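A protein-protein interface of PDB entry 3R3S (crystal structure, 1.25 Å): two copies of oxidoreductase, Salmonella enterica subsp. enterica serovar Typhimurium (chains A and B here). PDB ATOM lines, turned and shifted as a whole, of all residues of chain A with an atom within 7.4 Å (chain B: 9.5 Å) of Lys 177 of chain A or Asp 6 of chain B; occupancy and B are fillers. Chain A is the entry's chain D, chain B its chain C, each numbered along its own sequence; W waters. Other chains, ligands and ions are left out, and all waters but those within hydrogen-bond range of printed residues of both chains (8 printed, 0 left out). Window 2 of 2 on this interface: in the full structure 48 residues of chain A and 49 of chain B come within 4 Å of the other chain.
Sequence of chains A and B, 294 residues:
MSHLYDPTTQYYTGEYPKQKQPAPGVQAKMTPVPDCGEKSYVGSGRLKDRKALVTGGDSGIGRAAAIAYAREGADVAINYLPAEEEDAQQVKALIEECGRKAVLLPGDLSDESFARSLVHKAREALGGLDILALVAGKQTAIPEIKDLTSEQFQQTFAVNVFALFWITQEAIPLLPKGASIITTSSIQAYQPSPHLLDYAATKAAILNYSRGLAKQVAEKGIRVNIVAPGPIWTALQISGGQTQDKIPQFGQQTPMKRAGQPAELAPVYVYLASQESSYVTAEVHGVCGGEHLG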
ATOM      1  N   ASP A 130     -14.197 -10.330   3.863  1.00  0.00           N
ATOM      2  CA  ASP A 130     -12.863 -10.297   3.285  1.00  0.00           C
ATOM      3  C   ASP A 130     -11.999 -11.538   3.529  1.00  0.00           C
ATOM      4  O   ASP A 130     -10.844 -11.571   3.152  1.00  0.00           O
ATOM      5  CB  ASP A 130     -12.141  -9.007   3.716  1.00  0.00           C
ATOM      6  CG  ASP A 130     -12.105  -8.812   5.217  1.00  0.00           C
ATOM      7  OD1 ASP A 130     -11.797  -9.776   5.931  1.00  0.00           O
ATOM      8  OD2 ASP A 130     -12.403  -7.678   5.685  1.00  0.00           O
ATOM      9  N   LEU A 174     -17.928  -8.568  -4.972  1.00  0.00           N
ATOM     10  CA  LEU A 174     -18.094  -7.831  -3.725  1.00  0.00           C
ATOM     11  C   LEU A 174     -16.862  -7.856  -2.818  1.00  0.00           C
ATOM     12  O   LEU A 174     -16.817  -7.142  -1.817  1.00  0.00           O
ATOM     13  CB  LEU A 174     -19.363  -8.287  -2.972  1.00  0.00           C
ATOM     14  CG  LEU A 174     -19.616  -9.757  -2.653  1.00  0.00           C
ATOM     15  CD1 LEU A 174     -18.655 -10.255  -1.541  1.00  0.00           C
ATOM     16  CD2 LEU A 174     -21.089 -10.026  -2.268  1.00  0.00           C
ATOM     17  N   LEU A 175     -15.856  -8.646  -3.167  1.00  0.00           N
ATOM     18  CA  LEU A 175     -14.682  -8.754  -2.289  1.00  0.00           C
ATOM     19  C   LEU A 175     -13.747  -7.583  -2.519  1.00  0.00           C
ATOM     20  O   LEU A 175     -13.447  -7.232  -3.668  1.00  0.00           O
ATOM     21  CB  LEU A 175     -13.931 -10.060  -2.558  1.00  0.00           C
ATOM     22  CG  LEU A 175     -14.614 -11.319  -2.052  1.00  0.00           C
ATOM     23  CD1 LEU A 175     -13.828 -12.551  -2.534  1.00  0.00           C
ATOM     24  CD2 LEU A 175     -14.769 -11.308  -0.520  1.00  0.00           C
ATOM     25  N   PRO A 176     -13.240  -6.993  -1.432  1.00  0.00           N
ATOM     26  CA  PRO A 176     -12.291  -5.871  -1.550  1.00  0.00           C
ATOM     27  C   PRO A 176     -10.885  -6.336  -1.899  1.00  0.00           C
ATOM     28  O   PRO A 176     -10.530  -7.501  -1.716  1.00  0.00           O
ATOM     29  CB  PRO A 176     -12.311  -5.268  -0.145  1.00  0.00           C
ATOM     30  CG  PRO A 176     -12.557  -6.477   0.733  1.00  0.00           C
ATOM     31  CD  PRO A 176     -13.563  -7.316  -0.026  1.00  0.00           C
ATOM     32  N   LYS A 177     -10.094  -5.406  -2.404  1.00  0.00           N
ATOM     33  CA  LYS A 177      -8.660  -5.633  -2.536  1.00  0.00           C
ATOM     34  C   LYS A 177      -8.135  -6.075  -1.186  1.00  0.00           C
ATOM     35  O   LYS A 177      -8.483  -5.498  -0.151  1.00  0.00           O
ATOM     36  CB  LYS A 177      -7.951  -4.350  -2.971  1.00  0.00           C
ATOM     37  CG  LYS A 177      -8.414  -3.827  -4.316  1.00  0.00           C
ATOM     38  CD  LYS A 177      -7.795  -2.445  -4.617  1.00  0.00           C
ATOM     39  CE  LYS A 177      -8.309  -1.892  -5.935  1.00  0.00           C
ATOM     40  NZ  LYS A 177      -7.863  -0.471  -6.154  1.00  0.00           N
ATOM     41  N   GLY A 178      -7.288  -7.093  -1.187  1.00  0.00           N
ATOM     42  CA  GLY A 178      -6.793  -7.648   0.057  1.00  0.00           C
ATOM     43  C   GLY A 178      -7.566  -8.865   0.543  1.00  0.00           C
ATOM     44  O   GLY A 178      -7.108  -9.582   1.455  1.00  0.00           O
ATOM     45  N   ALA A 179      -8.726  -9.151  -0.049  1.00  0.00           N
ATOM     46  CA  ALA A 179      -9.501 -10.322   0.382  1.00  0.00           C
ATOM     47  C   ALA A 179      -8.745 -11.624   0.105  1.00  0.00           C
ATOM     48  O   ALA A 179      -7.930 -11.723  -0.849  1.00  0.00           O
ATOM     49  CB  ALA A 179     -10.856 -10.339  -0.299  1.00  0.00           C
ATOM     50  N   SER A 180      -9.005 -12.626   0.940  1.00  0.00           N
ATOM     51  CA  SER A 180      -8.301 -13.892   0.829  1.00  0.00           C
ATOM     52  C   SER A 180      -9.307 -15.050   0.834  1.00  0.00           C
ATOM     53  O   SER A 180     -10.159 -15.149   1.738  1.00  0.00           O
ATOM     54  CB  SER A 180      -7.342 -14.040   2.012  1.00  0.00           C
ATOM     55  OG  SER A 180      -6.607 -15.258   1.923  1.00  0.00           O
ATOM     56  N   ALA A 218      -6.196 -12.191  -9.543  1.00  0.00           N
ATOM     57  CA  ALA A 218      -5.013 -11.530  -9.002  1.00  0.00           C
ATOM     58  C   ALA A 218      -5.092 -10.015  -9.243  1.00  0.00           C
ATOM     59  O   ALA A 218      -4.756  -9.214  -8.358  1.00  0.00           O
ATOM     60  CB  ALA A 218      -3.756 -12.092  -9.641  1.00  0.00           C
ATOM     61  N   GLU A 219      -5.532  -9.613 -10.429  1.00  0.00           N
ATOM     62  CA  GLU A 219      -5.548  -8.184 -10.753  1.00  0.00           C
ATOM     63  C   GLU A 219      -6.536  -7.395  -9.895  1.00  0.00           C
ATOM     64  O   GLU A 219      -6.405  -6.172  -9.762  1.00  0.00           O
ATOM     65  CB  GLU A 219      -5.834  -7.974 -12.239  1.00  0.00           C
ATOM     66  CG  GLU A 219      -7.224  -8.394 -12.686  1.00  0.00           C
ATOM     67  CD  GLU A 219      -7.495  -8.035 -14.146  1.00  0.00           C
ATOM     68  OE1 GLU A 219      -6.595  -7.468 -14.818  1.00  0.00           O
ATOM     69  OE2 GLU A 219      -8.615  -8.324 -14.623  1.00  0.00           O
ATOM     70  N   LYS A 220      -7.518  -8.090  -9.320  1.00  0.00           N
ATOM     71  CA  LYS A 220      -8.515  -7.480  -8.437  1.00  0.00           C
ATOM     72  C   LYS A 220      -7.995  -7.417  -7.003  1.00  0.00           C
ATOM     73  O   LYS A 220      -8.708  -6.975  -6.095  1.00  0.00           O
ATOM     74  CB  LYS A 220      -9.834  -8.268  -8.457  1.00  0.00           C
ATOM     75  CG  LYS A 220     -10.480  -8.364  -9.849  1.00  0.00           C
ATOM     76  CD  LYS A 220     -11.763  -9.214  -9.807  1.00  0.00           C
ATOM     77  CE  LYS A 220     -12.303  -9.564 -11.203  1.00  0.00           C
ATOM     78  NZ  LYS A 220     -12.811  -8.358 -11.910  1.00  0.00           N
ATOM     79  N   GLY A 221      -6.753  -7.835  -6.779  1.00  0.00           N
ATOM     80  CA  GLY A 221      -6.202  -7.790  -5.435  1.00  0.00           C
ATOM     81  C   GLY A 221      -6.726  -8.863  -4.493  1.00  0.00           C
ATOM     82  O   GLY A 221      -6.574  -8.753  -3.270  1.00  0.00           O
ATOM     83  N   ILE A 222      -7.312  -9.922  -5.066  1.00  0.00           N
ATOM     84  CA  ILE A 222      -7.848 -11.036  -4.296  1.00  0.00           C
ATOM     85  C   ILE A 222      -6.877 -12.198  -4.437  1.00  0.00           C
ATOM     86  O   ILE A 222      -6.388 -12.443  -5.531  1.00  0.00           O
ATOM     87  CB  ILE A 222      -9.242 -11.441  -4.839  1.00  0.00           C
ATOM     88  CG1 ILE A 222     -10.227 -10.267  -4.692  1.00  0.00           C
ATOM     89  CG2 ILE A 222      -9.781 -12.647  -4.063  1.00  0.00           C
ATOM     90  CD1 ILE A 222     -11.474 -10.452  -5.539  1.00  0.00           C
ATOM     91  N   ARG A 223      -6.581 -12.893  -3.340  1.00  0.00           N
ATOM     92  CA  ARG A 223      -5.713 -14.092  -3.365  1.00  0.00           C
ATOM     93  C   ARG A 223      -6.580 -15.328  -3.158  1.00  0.00           C
ATOM     94  O   ARG A 223      -7.576 -15.278  -2.414  1.00  0.00           O
ATOM     95  CB  ARG A 223      -4.602 -14.011  -2.304  1.00  0.00           C
ATOM     96  CG  ARG A 223      -3.647 -12.827  -2.553  1.00  0.00           C
ATOM     97  CD  ARG A 223      -2.510 -12.748  -1.533  1.00  0.00           C
ATOM     98  NE  ARG A 223      -3.001 -12.515  -0.188  1.00  0.00           N
ATOM     99  CZ  ARG A 223      -3.075 -13.433   0.779  1.00  0.00           C
ATOM    100  NH1 ARG A 223      -2.680 -14.682   0.572  1.00  0.00           N
ATOM    101  NH2 ARG A 223      -3.586 -13.088   1.957  1.00  0.00           N
ATOM    102  N   GLN A 275      -2.883 -10.838   5.834  1.00  0.00           N
ATOM    103  CA  GLN A 275      -2.214 -10.021   4.824  1.00  0.00           C
ATOM    104  C   GLN A 275      -0.734 -10.364   4.703  1.00  0.00           C
ATOM    105  O   GLN A 275      -0.081 -10.006   3.715  1.00  0.00           O
ATOM    106  CB  GLN A 275      -2.356  -8.528   5.154  1.00  0.00           C
ATOM    107  CG  GLN A 275      -3.799  -8.053   5.306  1.00  0.00           C
ATOM    108  CD  GLN A 275      -3.881  -6.545   5.441  1.00  0.00           C
ATOM    109  OE1 GLN A 275      -3.264  -5.797   4.665  1.00  0.00           O
ATOM    110  NE2 GLN A 275      -4.618  -6.087   6.437  1.00  0.00           N
ATOM    111  N   SER A 278       1.009 -11.948   1.445  1.00  0.00           N
ATOM    112  CA  SER A 278       0.776 -11.088   0.299  1.00  0.00           C
ATOM    113  C   SER A 278       1.329 -11.590  -1.042  1.00  0.00           C
ATOM    114  O   SER A 278       0.785 -11.233  -2.077  1.00  0.00           O
ATOM    115  CB  SER A 278       1.371  -9.705   0.611  1.00  0.00           C
ATOM    116  OG  SER A 278       2.742  -9.793   1.014  1.00  0.00           O
ATOM    117  N   HIS B   3      -8.311  -1.671   7.013  1.00  0.00           N
ATOM    118  CA  HIS B   3      -6.859  -1.547   6.898  1.00  0.00           C
ATOM    119  C   HIS B   3      -6.332  -2.657   6.001  1.00  0.00           C
ATOM    120  O   HIS B   3      -5.244  -3.192   6.224  1.00  0.00           O
ATOM    121  CB  HIS B   3      -6.193  -1.610   8.280  1.00  0.00           C
ATOM    122  N   LEU B   4      -7.112  -2.989   4.980  1.00  0.00           N
ATOM    123  CA  LEU B   4      -6.714  -4.008   4.011  1.00  0.00           C
ATOM    124  C   LEU B   4      -5.959  -3.414   2.843  1.00  0.00           C
ATOM    125  O   LEU B   4      -6.431  -2.486   2.194  1.00  0.00           O
ATOM    126  CB  LEU B   4      -7.938  -4.716   3.452  1.00  0.00           C
ATOM    127  CG  LEU B   4      -8.352  -6.023   4.100  1.00  0.00           C
ATOM    128  CD1 LEU B   4      -9.491  -6.636   3.317  1.00  0.00           C
ATOM    129  CD2 LEU B   4      -7.169  -6.969   4.123  1.00  0.00           C
ATOM    130  N   TYR B   5      -4.791  -3.970   2.570  1.00  0.00           N
ATOM    131  CA  TYR B   5      -4.008  -3.480   1.416  1.00  0.00           C
ATOM    132  C   TYR B   5      -4.079  -4.412   0.203  1.00  0.00           C
ATOM    133  O   TYR B   5      -4.262  -5.609   0.329  1.00  0.00           O
ATOM    134  CB  TYR B   5      -2.558  -3.278   1.845  1.00  0.00           C
ATOM    135  CG  TYR B   5      -2.389  -2.187   2.887  1.00  0.00           C
ATOM    136  CD1 TYR B   5      -2.239  -0.855   2.516  1.00  0.00           C
ATOM    137  CD2 TYR B   5      -2.376  -2.491   4.244  1.00  0.00           C
ATOM    138  CE1 TYR B   5      -2.091   0.134   3.465  1.00  0.00           C
ATOM    139  CE2 TYR B   5      -2.218  -1.508   5.199  1.00  0.00           C
ATOM    140  CZ  TYR B   5      -2.080  -0.197   4.805  1.00  0.00           C
ATOM    141  OH  TYR B   5      -1.923   0.790   5.756  1.00  0.00           O
ATOM    142  N   ASP B   6      -3.928  -3.836  -0.970  1.00  0.00           N
ATOM    143  CA  ASP B   6      -3.910  -4.592  -2.212  1.00  0.00           C
ATOM    144  C   ASP B   6      -2.540  -5.226  -2.334  1.00  0.00           C
ATOM    145  O   ASP B   6      -1.527  -4.512  -2.450  1.00  0.00           O
ATOM    146  CB  ASP B   6      -4.110  -3.605  -3.369  1.00  0.00           C
ATOM    147  CG  ASP B   6      -4.217  -4.280  -4.717  1.00  0.00           C
ATOM    148  OD1 ASP B   6      -3.810  -5.448  -4.843  1.00  0.00           O
ATOM    149  OD2 ASP B   6      -4.735  -3.639  -5.658  1.00  0.00           O
ATOM    150  N   PRO B   7      -2.478  -6.564  -2.321  1.00  0.00           N
ATOM    151  CA  PRO B   7      -1.140  -7.172  -2.367  1.00  0.00           C
ATOM    152  C   PRO B   7      -0.405  -6.894  -3.690  1.00  0.00           C
ATOM    153  O   PRO B   7       0.830  -6.937  -3.732  1.00  0.00           O
ATOM    154  CB  PRO B   7      -1.433  -8.675  -2.141  1.00  0.00           C
ATOM    155  CG  PRO B   7      -2.824  -8.851  -2.625  1.00  0.00           C
ATOM    156  CD  PRO B   7      -3.555  -7.573  -2.275  1.00  0.00           C
ATOM    157  N   THR B   8      -1.135  -6.607  -4.762  1.00  0.00           N
ATOM    158  CA  THR B   8      -0.448  -6.353  -6.032  1.00  0.00           C
ATOM    159  C   THR B   8       0.397  -5.089  -6.008  1.00  0.00           C
ATOM    160  O   THR B   8       1.425  -5.026  -6.701  1.00  0.00           O
ATOM    161  CB  THR B   8      -1.383  -6.340  -7.249  1.00  0.00           C
ATOM    162  OG1 THR B   8      -2.299  -5.253  -7.125  1.00  0.00           O
ATOM    163  CG2 THR B   8      -2.124  -7.673  -7.401  1.00  0.00           C
ATOM    164  N   THR B   9      -0.013  -4.097  -5.217  1.00  0.00           N
ATOM    165  CA  THR B   9       0.696  -2.824  -5.163  1.00  0.00           C
ATOM    166  C   THR B   9       1.406  -2.549  -3.841  1.00  0.00           C
ATOM    167  O   THR B   9       1.999  -1.470  -3.673  1.00  0.00           O
ATOM    168  CB  THR B   9      -0.235  -1.652  -5.469  1.00  0.00           C
ATOM    169  OG1 THR B   9      -1.285  -1.645  -4.506  1.00  0.00           O
ATOM    170  CG2 THR B   9      -0.831  -1.773  -6.861  1.00  0.00           C
ATOM    171  N   GLN B  10       1.418  -3.538  -2.944  1.00  0.00           N
ATOM    172  CA  GLN B  10       1.978  -3.339  -1.622  1.00  0.00           C
ATOM    173  C   GLN B  10       3.477  -3.122  -1.661  1.00  0.00           C
ATOM    174  O   GLN B  10       4.043  -2.465  -0.779  1.00  0.00           O
ATOM    175  CB  GLN B  10       1.641  -4.538  -0.744  1.00  0.00           C
ATOM    176  CG  GLN B  10       2.094  -4.358   0.669  1.00  0.00           C
ATOM    177  CD  GLN B  10       1.614  -5.514   1.494  1.00  0.00           C
ATOM    178  OE1 GLN B  10       0.777  -6.316   1.030  1.00  0.00           O
ATOM    179  NE2 GLN B  10       2.126  -5.629   2.713  1.00  0.00           N
ATOM    180  N   TYR B  11       4.114  -3.713  -2.664  1.00  0.00           N
ATOM    181  CA  TYR B  11       5.552  -3.578  -2.882  1.00  0.00           C
ATOM    182  C   TYR B  11       5.790  -3.111  -4.296  1.00  0.00           C
ATOM    183  O   TYR B  11       4.877  -3.086  -5.131  1.00  0.00           O
ATOM    184  CB  TYR B  11       6.241  -4.925  -2.637  1.00  0.00           C
ATOM    185  CG  TYR B  11       6.229  -5.347  -1.184  1.00  0.00           C
ATOM    186  CD1 TYR B  11       5.265  -6.229  -0.709  1.00  0.00           C
ATOM    187  CD2 TYR B  11       7.140  -4.815  -0.278  1.00  0.00           C
ATOM    188  CE1 TYR B  11       5.238  -6.590   0.623  1.00  0.00           C
ATOM    189  CE2 TYR B  11       7.128  -5.172   1.059  1.00  0.00           C
ATOM    190  CZ  TYR B  11       6.173  -6.064   1.501  1.00  0.00           C
ATOM    191  OH  TYR B  11       6.116  -6.464   2.825  1.00  0.00           O
ATOM    192  N   TYR B  12       7.025  -2.697  -4.565  1.00  0.00           N
ATOM    193  CA  TYR B  12       7.387  -2.044  -5.806  1.00  0.00           C
ATOM    194  C   TYR B  12       6.949  -2.840  -7.026  1.00  0.00           C
ATOM    195  O   TYR B  12       7.261  -4.023  -7.133  1.00  0.00           O
ATOM    196  CB  TYR B  12       8.907  -1.792  -5.813  1.00  0.00           C
ATOM    197  CG  TYR B  12       9.384  -1.106  -7.070  1.00  0.00           C
ATOM    198  CD1 TYR B  12       8.902   0.166  -7.455  1.00  0.00           C
ATOM    199  CD2 TYR B  12      10.290  -1.752  -7.911  1.00  0.00           C
ATOM    200  CE1 TYR B  12       9.368   0.786  -8.618  1.00  0.00           C
ATOM    201  CE2 TYR B  12      10.764  -1.144  -9.070  1.00  0.00           C
ATOM    202  CZ  TYR B  12      10.268   0.116  -9.428  1.00  0.00           C
ATOM    203  OH  TYR B  12      10.671   0.727 -10.594  1.00  0.00           O
ATOM    204  N   THR B  13       6.277  -2.168  -7.963  1.00  0.00           N
ATOM    205  CA  THR B  13       5.707  -2.823  -9.154  1.00  0.00           C
ATOM    206  C   THR B  13       6.396  -2.411 -10.442  1.00  0.00           C
ATOM    207  O   THR B  13       6.059  -2.911 -11.506  1.00  0.00           O
ATOM    208  CB  THR B  13       4.207  -2.468  -9.324  1.00  0.00           C
ATOM    209  OG1 THR B  13       4.092  -1.088  -9.720  1.00  0.00           O
ATOM    210  CG2 THR B  13       3.435  -2.732  -8.027  1.00  0.00           C
ATOM    211  N   PRO B 255       1.347 -13.641 -12.088  1.00  0.00           N
ATOM    212  CA  PRO B 255      -0.030 -13.123 -12.042  1.00  0.00           C
ATOM    213  C   PRO B 255      -0.128 -11.820 -11.238  1.00  0.00           C
ATOM    214  O   PRO B 255      -0.926 -10.932 -11.576  1.00  0.00           O
ATOM    215  CB  PRO B 255      -0.804 -14.272 -11.398  1.00  0.00           C
ATOM    216  CG  PRO B 255      -0.081 -15.474 -11.910  1.00  0.00           C
ATOM    217  CD  PRO B 255       1.384 -15.097 -11.874  1.00  0.00           C
ATOM    218  N   MET B 256       0.669 -11.679 -10.183  1.00  0.00           N
ATOM    219  CA  MET B 256       0.609 -10.441  -9.423  1.00  0.00           C
ATOM    220  C   MET B 256       1.322  -9.259 -10.087  1.00  0.00           C
ATOM    221  O   MET B 256       1.198  -8.140  -9.578  1.00  0.00           O
ATOM    222  CB  MET B 256       1.154 -10.655  -8.028  1.00  0.00           C
ATOM    223  CG  MET B 256       0.219 -11.519  -7.200  1.00  0.00           C
ATOM    224  SD  MET B 256       0.680 -11.462  -5.472  1.00  0.00           S
ATOM    225  CE  MET B 256      -0.753 -12.215  -4.770  1.00  0.00           C
ATOM    226  N   ARG B 258       4.433  -8.342 -10.299  1.00  0.00           N
ATOM    227  CA  ARG B 258       5.596  -7.752  -9.661  1.00  0.00           C
ATOM    228  C   ARG B 258       6.442  -8.878  -9.090  1.00  0.00           C
ATOM    229  O   ARG B 258       5.930  -9.983  -8.836  1.00  0.00           O
ATOM    230  CB  ARG B 258       5.184  -6.766  -8.560  1.00  0.00           C
ATOM    231  CG  ARG B 258       4.449  -7.429  -7.405  1.00  0.00           C
ATOM    232  CD  ARG B 258       4.372  -6.479  -6.183  1.00  0.00           C
ATOM    233  NE  ARG B 258       3.581  -7.012  -5.085  1.00  0.00           N
ATOM    234  CZ  ARG B 258       4.072  -7.784  -4.106  1.00  0.00           C
ATOM    235  NH1 ARG B 258       5.354  -8.138  -4.094  1.00  0.00           N
ATOM    236  NH2 ARG B 258       3.271  -8.229  -3.142  1.00  0.00           N
ATOM    237  N   GLU B 264       8.374 -10.822   2.256  1.00  0.00           N
ATOM    238  CA  GLU B 264       7.197 -11.625   2.038  1.00  0.00           C
ATOM    239  C   GLU B 264       7.417 -13.127   2.248  1.00  0.00           C
ATOM    240  O   GLU B 264       6.462 -13.917   2.226  1.00  0.00           O
ATOM    241  CB  GLU B 264       6.645 -11.315   0.644  1.00  0.00           C
ATOM    242  CG  GLU B 264       6.242  -9.838   0.501  1.00  0.00           C
ATOM    243  CD  GLU B 264       5.662  -9.560  -0.880  1.00  0.00           C
ATOM    244  OE1 GLU B 264       6.466  -9.405  -1.849  1.00  0.00           O
ATOM    245  OE2 GLU B 264       4.407  -9.557  -0.992  1.00  0.00           O
HETATM  246  O   HOH W   1      -6.482  -4.338  -7.609  1.00  0.00           O
HETATM  247  O   HOH W   2      -9.163  -2.919   0.502  1.00  0.00           O
HETATM  248  O   HOH W   3      -2.358  -8.553 -11.253  1.00  0.00           O
HETATM  249  O   HOH W   4       3.563  -8.277   3.140  1.00  0.00           O
HETATM  250  O   HOH W   5      -4.830  -0.964  -5.830  1.00  0.00           O
HETATM  251  O   HOH W   6       3.834 -13.309   1.450  1.00  0.00           O
HETATM  252  O   HOH W   7      -3.423  -4.754  -9.557  1.00  0.00           O
HETATM  253  O   HOH W   8       1.825  -7.701   4.692  1.00  0.00           O
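No position is printed for both chains.
The side-chain carboxylate (OE2) of Glu 264 of chain B is in hydrogen-bond range of the side-chain hydroxyl (OG) of Ser 278 of chain A. The side-chain amide nitrogen of Gln 275 of chain A sits at hydrogen-bond distance from the backbone carbonyl oxygen of His 3 of chain B (3.0 Å). The side-chain sulfur (SD) of Met 256 of chain B lies close to the backbone carbonyl oxygen (O) of Ser 278 of chain A (3.4 Å). The side-chain amide oxygen (OE1) of Gln 275 of chain A sits at hydrogen-bond distance from the backbone NH (N) of Tyr 5 of chain B (3.2 Å).
Water W5 bridges OD2 of Asp 6 of chain B (2.7 Å) and NZ of Lys 177 of chain A (3.1 Å). Water W1 lies within hydrogen-bond range of the side-chain carboxylate of Asp 6 of chain B and the backbone carbonyl oxygen of Glu 219 of chain A. Water W7 bridges the side-chain hydroxyl (OG1) of Thr 8 of chain B (2.7 Å) and the backbone carbonyl oxygen (O) of Glu 219 of chain A (3.3 Å). Water W4 lies within hydrogen-bond range of the side-chain hydroxyl (OG) of Ser 278 of chain A (2.7 Å), the side-chain amide nitrogen (NE2) of Gln 10 of chain B (3.0 Å) and the side-chain hydroxyl (OH) of Tyr 11 of chain B (3.1 Å). Water W3 bridges O of Pro 255 of chain B (2.8 Å) and N of Glu 219 of chain A (3.4 Å). Water W8 bridges NE2 of Gln 10 of chain B and O of Gln 275 of chain A.
Of the 15 printed residues of chain B, 10 touch a printed residue of chain A. Hydrophobic or aromatic side chains of chain A within 4 Å of the printed part of chain B: Ala 218. Among the printed residues, 18 pairs touch across the chains.
Of the printed residues of chain B, Asp 130 of chain A touches Leu 4. Lys 177 of chain A touches just these residues of chain B: Leu 4 (3.7 Å) and Asp 6 (3.4 Å). Asp 6 of chain B touches just these residues of chain A: Lys 177 and Gly 221. Printed residues of chain A within 4 Å of Gln 10 of chain B: Ser 278. The nearest printed residue of chain B that does not touch Lys 177 of chain A is Tyr 5 of chain B (4.2 Å). The nearest printed residue of chain A that does not touch Leu 4 of chain B is Pro 176 of chain A (4.01 Å).
CD1 of Leu 4 of chain B touches CB of Asp 130 of chain A, at 3.6 Å. Lys 177 of chain A touches Asp 6 of chain B (CD to OD2, 3.4 Å). Leu 4 of chain B touches Gly 178 of chain A. Gly 178 of chain A touches Pro 7 of chain B (N to CD, 3.9 Å). Ala 218 of chain A touches Thr 8 of chain B (O to CG2, 3.2 Å). Ala 218 of chain A touches Pro 255 of chain B. O of Gly 221 of chain A touches CD of Pro 7 of chain B (3.4 Å). CG of Arg 223 of chain A touches CE of Met 256 of chain B, 3.7 Å away. O of Ser 278 of chain A touches CB of Pro 7 of chain B (3.4 Å). Ser 278 of chain A touches Gln 10 of chain B (CB to OE1, 3.5 Å).
The backbone NH of Arg 223 of chain A sits at hydrogen-bond distance from the backbone carbonyl oxygen of Ala 179 of chain A (3.1 Å). The guanidinium group of Arg 258 of chain B lies within hydrogen-bond range of the backbone carbonyl oxygen of Pro 7 of chain B. The guanidinium group (NE) of Arg 258 of chain B sits close to the backbone carbonyl oxygen (O) of Thr 8 of chain B, 3.3 Å away. N of Gly 178 of chain A sits at hydrogen-bond distance from O of Gly 221 of chain A (2.8 Å). NH2 of Arg 258 of chain B is in salt-bridge range of OE2 of Glu 264 of chain B, 2.8 Å away. The backbone carbonyl oxygen (O) of Asp 130 of chain A is in hydrogen-bond range of the backbone NH (N) of Ser 180 of chain A (3.1 Å).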
